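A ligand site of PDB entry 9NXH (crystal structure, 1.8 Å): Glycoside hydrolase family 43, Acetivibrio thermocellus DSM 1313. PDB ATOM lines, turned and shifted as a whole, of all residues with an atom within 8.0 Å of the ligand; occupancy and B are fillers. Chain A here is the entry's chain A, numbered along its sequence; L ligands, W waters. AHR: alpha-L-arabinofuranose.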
ATOM      1  N   SER A  13       9.122   0.344  28.657  1.00  0.00           N
ATOM      2  CA  SER A  13       9.296  -0.093  27.265  1.00  0.00           C
ATOM      3  C   SER A  13       9.467   1.111  26.336  1.00  0.00           C
ATOM      4  O   SER A  13       8.813   2.143  26.509  1.00  0.00           O
ATOM      5  CB  SER A  13       8.087  -0.929  26.833  1.00  0.00           C
ATOM      6  OG  SER A  13       8.031  -1.026  25.423  1.00  0.00           O
ATOM      7  N   ASN A  15       8.819   1.043  22.937  1.00  0.00           N
ATOM      8  CA  ASN A  15       7.722   1.146  21.984  1.00  0.00           C
ATOM      9  C   ASN A  15       6.341   1.127  22.635  1.00  0.00           C
ATOM     10  O   ASN A  15       5.367   1.570  21.996  1.00  0.00           O
ATOM     11  CB  ASN A  15       7.812   0.060  20.884  1.00  0.00           C
ATOM     12  CG  ASN A  15       8.141  -1.335  21.411  1.00  0.00           C
ATOM     13  OD1 ASN A  15       8.465  -1.551  22.582  1.00  0.00           O
ATOM     14  ND2 ASN A  15       8.076  -2.327  20.500  1.00  0.00           N
ATOM     15  N   TYR A  16       6.239   0.673  23.878  1.00  0.00           N
ATOM     16  CA  TYR A  16       5.003   0.771  24.672  1.00  0.00           C
ATOM     17  C   TYR A  16       5.355   1.536  25.942  1.00  0.00           C
ATOM     18  O   TYR A  16       5.572   0.934  26.992  1.00  0.00           O
ATOM     19  CB  TYR A  16       4.423  -0.618  24.983  1.00  0.00           C
ATOM     20  CG  TYR A  16       4.029  -1.319  23.713  1.00  0.00           C
ATOM     21  CD1 TYR A  16       2.729  -1.226  23.233  1.00  0.00           C
ATOM     22  CD2 TYR A  16       4.962  -2.011  22.963  1.00  0.00           C
ATOM     23  CE1 TYR A  16       2.356  -1.839  22.056  1.00  0.00           C
ATOM     24  CE2 TYR A  16       4.605  -2.648  21.767  1.00  0.00           C
ATOM     25  CZ  TYR A  16       3.293  -2.547  21.329  1.00  0.00           C
ATOM     26  OH  TYR A  16       2.899  -3.150  20.154  1.00  0.00           O
ATOM     27  N   MET A  19       4.069   1.038  29.442  1.00  0.00           N
ATOM     28  CA  MET A  19       4.247  -0.276  30.024  1.00  0.00           C
ATOM     29  C   MET A  19       5.640  -0.434  30.608  1.00  0.00           C
ATOM     30  O   MET A  19       6.615   0.153  30.121  1.00  0.00           O
ATOM     31  CB  MET A  19       3.989  -1.381  28.988  1.00  0.00           C
ATOM     32  CG  MET A  19       2.587  -1.315  28.436  1.00  0.00           C
ATOM     33  SD  MET A  19       2.314  -2.753  27.362  1.00  0.00           S
ATOM     34  CE  MET A  19       0.669  -2.370  26.778  1.00  0.00           C
ATOM     35  N   ILE A  30       5.544  -7.208  30.731  1.00  0.00           N
ATOM     36  CA  ILE A  30       5.304  -5.769  30.717  1.00  0.00           C
ATOM     37  C   ILE A  30       3.796  -5.536  30.790  1.00  0.00           C
ATOM     38  O   ILE A  30       3.001  -6.255  30.177  1.00  0.00           O
ATOM     39  CB  ILE A  30       5.908  -5.056  29.491  1.00  0.00           C
ATOM     40  CG1 ILE A  30       5.312  -5.583  28.169  1.00  0.00           C
ATOM     41  CG2 ILE A  30       7.448  -5.182  29.489  1.00  0.00           C
ATOM     42  CD1 ILE A  30       5.709  -4.747  26.960  1.00  0.00           C
ATOM     43  N   ARG A 117      14.206  -8.708  25.825  1.00  0.00           N
ATOM     44  CA  ARG A 117      13.190  -8.125  24.950  1.00  0.00           C
ATOM     45  C   ARG A 117      11.819  -8.626  25.375  1.00  0.00           C
ATOM     46  O   ARG A 117      11.694  -9.693  25.990  1.00  0.00           O
ATOM     47  CB  ARG A 117      13.414  -8.470  23.467  1.00  0.00           C
ATOM     48  CG  ARG A 117      13.297  -9.971  23.105  1.00  0.00           C
ATOM     49  CD  ARG A 117      11.867 -10.390  22.690  1.00  0.00           C
ATOM     50  NE  ARG A 117      11.359  -9.647  21.536  1.00  0.00           N
ATOM     51  CZ  ARG A 117      11.659  -9.934  20.271  1.00  0.00           C
ATOM     52  NH1 ARG A 117      12.459 -10.972  20.009  1.00  0.00           N
ATOM     53  NH2 ARG A 117      11.179  -9.189  19.280  1.00  0.00           N
ATOM     54  N   HIS A 118      10.795  -7.873  25.005  1.00  0.00           N
ATOM     55  CA  HIS A 118       9.440  -8.336  25.243  1.00  0.00           C
ATOM     56  C   HIS A 118       8.803  -8.860  23.956  1.00  0.00           C
ATOM     57  O   HIS A 118       9.061  -8.340  22.864  1.00  0.00           O
ATOM     58  CB  HIS A 118       8.564  -7.250  25.867  1.00  0.00           C
ATOM     59  CG  HIS A 118       8.310  -6.065  24.989  1.00  0.00           C
ATOM     60  ND1 HIS A 118       7.249  -6.013  24.108  1.00  0.00           N
ATOM     61  CD2 HIS A 118       8.949  -4.881  24.873  1.00  0.00           C
ATOM     62  CE1 HIS A 118       7.266  -4.856  23.469  1.00  0.00           C
ATOM     63  NE2 HIS A 118       8.289  -4.146  23.923  1.00  0.00           N
ATOM     64  N   TYR A 119       7.971  -9.877  24.109  1.00  0.00           N
ATOM     65  CA  TYR A 119       7.249 -10.479  22.990  1.00  0.00           C
ATOM     66  C   TYR A 119       5.937 -11.057  23.507  1.00  0.00           C
ATOM     67  O   TYR A 119       5.958 -11.867  24.444  1.00  0.00           O
ATOM     68  CB  TYR A 119       8.098 -11.558  22.315  1.00  0.00           C
ATOM     69  CG  TYR A 119       7.299 -12.419  21.377  1.00  0.00           C
ATOM     70  CD1 TYR A 119       6.798 -11.890  20.202  1.00  0.00           C
ATOM     71  CD2 TYR A 119       7.010 -13.735  21.698  1.00  0.00           C
ATOM     72  CE1 TYR A 119       6.019 -12.668  19.345  1.00  0.00           C
ATOM     73  CE2 TYR A 119       6.245 -14.525  20.847  1.00  0.00           C
ATOM     74  CZ  TYR A 119       5.754 -13.981  19.681  1.00  0.00           C
ATOM     75  OH  TYR A 119       4.987 -14.764  18.819  1.00  0.00           O
ATOM     76  N   ASN A 120       4.817 -10.642  22.926  1.00  0.00           N
ATOM     77  CA  ASN A 120       3.485 -10.945  23.481  1.00  0.00           C
ATOM     78  C   ASN A 120       3.415 -10.569  24.961  1.00  0.00           C
ATOM     79  O   ASN A 120       2.776 -11.224  25.779  1.00  0.00           O
ATOM     80  CB  ASN A 120       3.113 -12.417  23.254  1.00  0.00           C
ATOM     81  CG  ASN A 120       2.792 -12.693  21.790  1.00  0.00           C
ATOM     82  OD1 ASN A 120       2.516 -11.763  21.032  1.00  0.00           O
ATOM     83  ND2 ASN A 120       2.863 -13.963  21.384  1.00  0.00           N
ATOM     84  N   TYR A 121       4.102  -9.472  25.290  1.00  0.00           N
ATOM     85  CA  TYR A 121       4.176  -8.870  26.624  1.00  0.00           C
ATOM     86  C   TYR A 121       4.946  -9.704  27.634  1.00  0.00           C
ATOM     87  O   TYR A 121       5.034  -9.307  28.796  1.00  0.00           O
ATOM     88  CB  TYR A 121       2.791  -8.532  27.185  1.00  0.00           C
ATOM     89  CG  TYR A 121       1.989  -7.647  26.252  1.00  0.00           C
ATOM     90  CD1 TYR A 121       2.480  -6.412  25.848  1.00  0.00           C
ATOM     91  CD2 TYR A 121       0.763  -8.060  25.762  1.00  0.00           C
ATOM     92  CE1 TYR A 121       1.755  -5.604  24.969  1.00  0.00           C
ATOM     93  CE2 TYR A 121       0.027  -7.262  24.886  1.00  0.00           C
ATOM     94  CZ  TYR A 121       0.528  -6.041  24.497  1.00  0.00           C
ATOM     95  OH  TYR A 121      -0.203  -5.264  23.632  1.00  0.00           O
ATOM     96  N   LEU A 122       5.548 -10.827  27.250  1.00  0.00           N
ATOM     97  CA  LEU A 122       6.386 -11.607  28.147  1.00  0.00           C
ATOM     98  C   LEU A 122       7.852 -11.291  27.873  1.00  0.00           C
ATOM     99  O   LEU A 122       8.215 -10.817  26.800  1.00  0.00           O
ATOM    100  CB  LEU A 122       6.116 -13.108  27.977  1.00  0.00           C
ATOM    101  CG  LEU A 122       4.648 -13.480  28.237  1.00  0.00           C
ATOM    102  CD1 LEU A 122       4.378 -14.944  27.919  1.00  0.00           C
ATOM    103  CD2 LEU A 122       4.305 -13.160  29.663  1.00  0.00           C
ATOM    104  N   LEU A 123       8.710 -11.547  28.855  1.00  0.00           N
ATOM    105  CA  LEU A 123      10.123 -11.235  28.727  1.00  0.00           C
ATOM    106  C   LEU A 123      10.912 -12.456  28.259  1.00  0.00           C
ATOM    107  O   LEU A 123      10.733 -13.560  28.771  1.00  0.00           O
ATOM    108  CB  LEU A 123      10.705 -10.732  30.036  1.00  0.00           C
ATOM    109  CG  LEU A 123      10.758  -9.240  30.367  1.00  0.00           C
ATOM    110  CD1 LEU A 123      11.988  -9.020  31.261  1.00  0.00           C
ATOM    111  CD2 LEU A 123      10.833  -8.358  29.133  1.00  0.00           C
ATOM    112  N   THR A 130      15.469  -7.499  13.670  1.00  0.00           N
ATOM    113  CA  THR A 130      14.592  -6.560  12.979  1.00  0.00           C
ATOM    114  C   THR A 130      14.459  -5.247  13.766  1.00  0.00           C
ATOM    115  O   THR A 130      14.843  -5.153  14.926  1.00  0.00           O
ATOM    116  CB  THR A 130      13.210  -7.160  12.733  1.00  0.00           C
ATOM    117  OG1 THR A 130      12.572  -7.440  13.989  1.00  0.00           O
ATOM    118  CG2 THR A 130      13.289  -8.471  11.888  1.00  0.00           C
ATOM    119  N   LEU A 132      11.627  -4.182  14.710  1.00  0.00           N
ATOM    120  CA  LEU A 132      10.718  -4.605  15.772  1.00  0.00           C
ATOM    121  C   LEU A 132      11.500  -5.157  16.952  1.00  0.00           C
ATOM    122  O   LEU A 132      11.320  -4.724  18.097  1.00  0.00           O
ATOM    123  CB  LEU A 132       9.722  -5.634  15.238  1.00  0.00           C
ATOM    124  CG  LEU A 132       8.809  -6.302  16.277  1.00  0.00           C
ATOM    125  CD1 LEU A 132       7.876  -5.322  17.046  1.00  0.00           C
ATOM    126  CD2 LEU A 132       8.005  -7.425  15.627  1.00  0.00           C
ATOM    127  N   ASP A 133      12.410  -6.105  16.672  1.00  0.00           N
ATOM    128  CA  ASP A 133      13.269  -6.644  17.734  1.00  0.00           C
ATOM    129  C   ASP A 133      13.988  -5.525  18.474  1.00  0.00           C
ATOM    130  O   ASP A 133      14.067  -5.543  19.705  1.00  0.00           O
ATOM    131  CB  ASP A 133      14.315  -7.606  17.151  1.00  0.00           C
ATOM    132  CG  ASP A 133      13.733  -8.859  16.502  1.00  0.00           C
ATOM    133  OD1 ASP A 133      12.595  -9.273  16.817  1.00  0.00           O
ATOM    134  OD2 ASP A 133      14.477  -9.466  15.687  1.00  0.00           O
ATOM    135  N   GLU A 135      13.218  -2.384  18.917  1.00  0.00           N
ATOM    136  CA  GLU A 135      12.341  -1.631  19.813  1.00  0.00           C
ATOM    137  C   GLU A 135      11.912  -2.485  20.997  1.00  0.00           C
ATOM    138  O   GLU A 135      11.805  -1.977  22.121  1.00  0.00           O
ATOM    139  CB  GLU A 135      11.136  -1.084  19.052  1.00  0.00           C
ATOM    140  CG  GLU A 135      11.512  -0.169  17.884  1.00  0.00           C
ATOM    141  CD  GLU A 135      10.472   0.899  17.591  1.00  0.00           C
ATOM    142  OE1 GLU A 135      10.763   1.790  16.762  1.00  0.00           O
ATOM    143  OE2 GLU A 135       9.387   0.871  18.210  1.00  0.00           O
ATOM    144  N   ASP A 136      11.651  -3.781  20.760  1.00  0.00           N
ATOM    145  CA  ASP A 136      11.272  -4.694  21.842  1.00  0.00           C
ATOM    146  C   ASP A 136      12.382  -4.881  22.855  1.00  0.00           C
ATOM    147  O   ASP A 136      12.121  -5.387  23.949  1.00  0.00           O
ATOM    148  CB  ASP A 136      10.927  -6.085  21.300  1.00  0.00           C
ATOM    149  CG  ASP A 136       9.577  -6.153  20.594  1.00  0.00           C
ATOM    150  OD1 ASP A 136       8.762  -5.203  20.693  1.00  0.00           O
ATOM    151  OD2 ASP A 136       9.354  -7.172  19.926  1.00  0.00           O
ATOM    152  N   ALA A 137      13.622  -4.536  22.493  1.00  0.00           N
ATOM    153  CA  ALA A 137      14.786  -4.724  23.348  1.00  0.00           C
ATOM    154  C   ALA A 137      15.296  -3.413  23.927  1.00  0.00           C
ATOM    155  O   ALA A 137      16.388  -3.400  24.517  1.00  0.00           O
ATOM    156  CB  ALA A 137      15.899  -5.429  22.576  1.00  0.00           C
HETATM  157  O5  AHR L   1       5.237  -7.783  23.577  1.00  0.00           O
HETATM  158  C5  AHR L   1       4.426  -6.884  22.846  1.00  0.00           C
HETATM  159  C4  AHR L   1       4.555  -7.146  21.358  1.00  0.00           C
HETATM  160  O4  AHR L   1       4.163  -8.499  21.060  1.00  0.00           O
HETATM  161  C3  AHR L   1       5.962  -6.984  20.769  1.00  0.00           C
HETATM  162  O3  AHR L   1       6.187  -5.630  20.381  1.00  0.00           O
HETATM  163  C2  AHR L   1       5.921  -7.934  19.569  1.00  0.00           C
HETATM  164  O2  AHR L   1       7.153  -8.575  19.336  1.00  0.00           O
HETATM  165  C1  AHR L   1       4.766  -8.911  19.840  1.00  0.00           C
HETATM  166  O1  AHR L   1       3.869  -8.787  18.789  1.00  0.00           O
HETATM  167  O   HOH W   1       4.679  -4.355  18.725  1.00  0.00           O
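Merely in contact with the ligand: Asn 15 (3.8 Å), Tyr 16 (3.6 Å) and Leu 132 (3.8 Å). Hydrophobic or aromatic side chains that line the ligand: Tyr 16, His 118, Tyr 119, Tyr 121 and Leu 132. Within 4 Å of the ligand: Asn 15, Tyr 16, His 118, Tyr 119, Asn 120, Tyr 121, Leu 132 and Asp 136.
The side-chain carboxylate of Asp 136 lies within hydrogen-bond range of an oxygen (O3) of the ligand (2.6 Å). The backbone NH (N) of Tyr 121 sits at hydrogen-bond distance from an oxygen (O5) of the ligand (2.7 Å). ND1 of His 118 is in hydrogen-bond range of O5 of the ligand (2.7 Å). An oxygen (O4) of the ligand lies within hydrogen-bond range of the backbone NH (N) of Asn 120, at 2.9 Å. The backbone NH (N) of Tyr 119 sits close to an oxygen (O5) of the ligand (3.5 Å).
The guanidinium group (NH2) of Arg 117 is in salt-bridge range of the side-chain carboxylate (OD2) of Asp 136, at 2.8 Å. The backbone carbonyl oxygen (O) of Tyr 121 is in hydrogen-bond range of the backbone NH (N) of Ile 30, 2.9 Å away. A ring nitrogen (NE2) of His 118 sits at hydrogen-bond distance from the side-chain hydroxyl (OG) of Ser 13, at 3.5 Å. The side-chain amide nitrogen (ND2) of Asn 120 sits close to the side-chain hydroxyl (OH) of Tyr 119. N of Tyr 16 is in hydrogen-bond range of OG of Ser 13, 2.9 Å away. The backbone NH (N) of Leu 132 sits close to the side-chain hydroxyl (OG1) of Thr 130 (3.5 Å). The side-chain amide oxygen (OD1) of Asn 15 lies close to the backbone carbonyl oxygen (O) of Glu 135, 3.4 Å away. OG of Ser 13 lies within hydrogen-bond range of OD1 of Asn 15 (2.9 Å).
Water W1 lies within hydrogen-bond range of O3 of the ligand and OH of Tyr 16.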
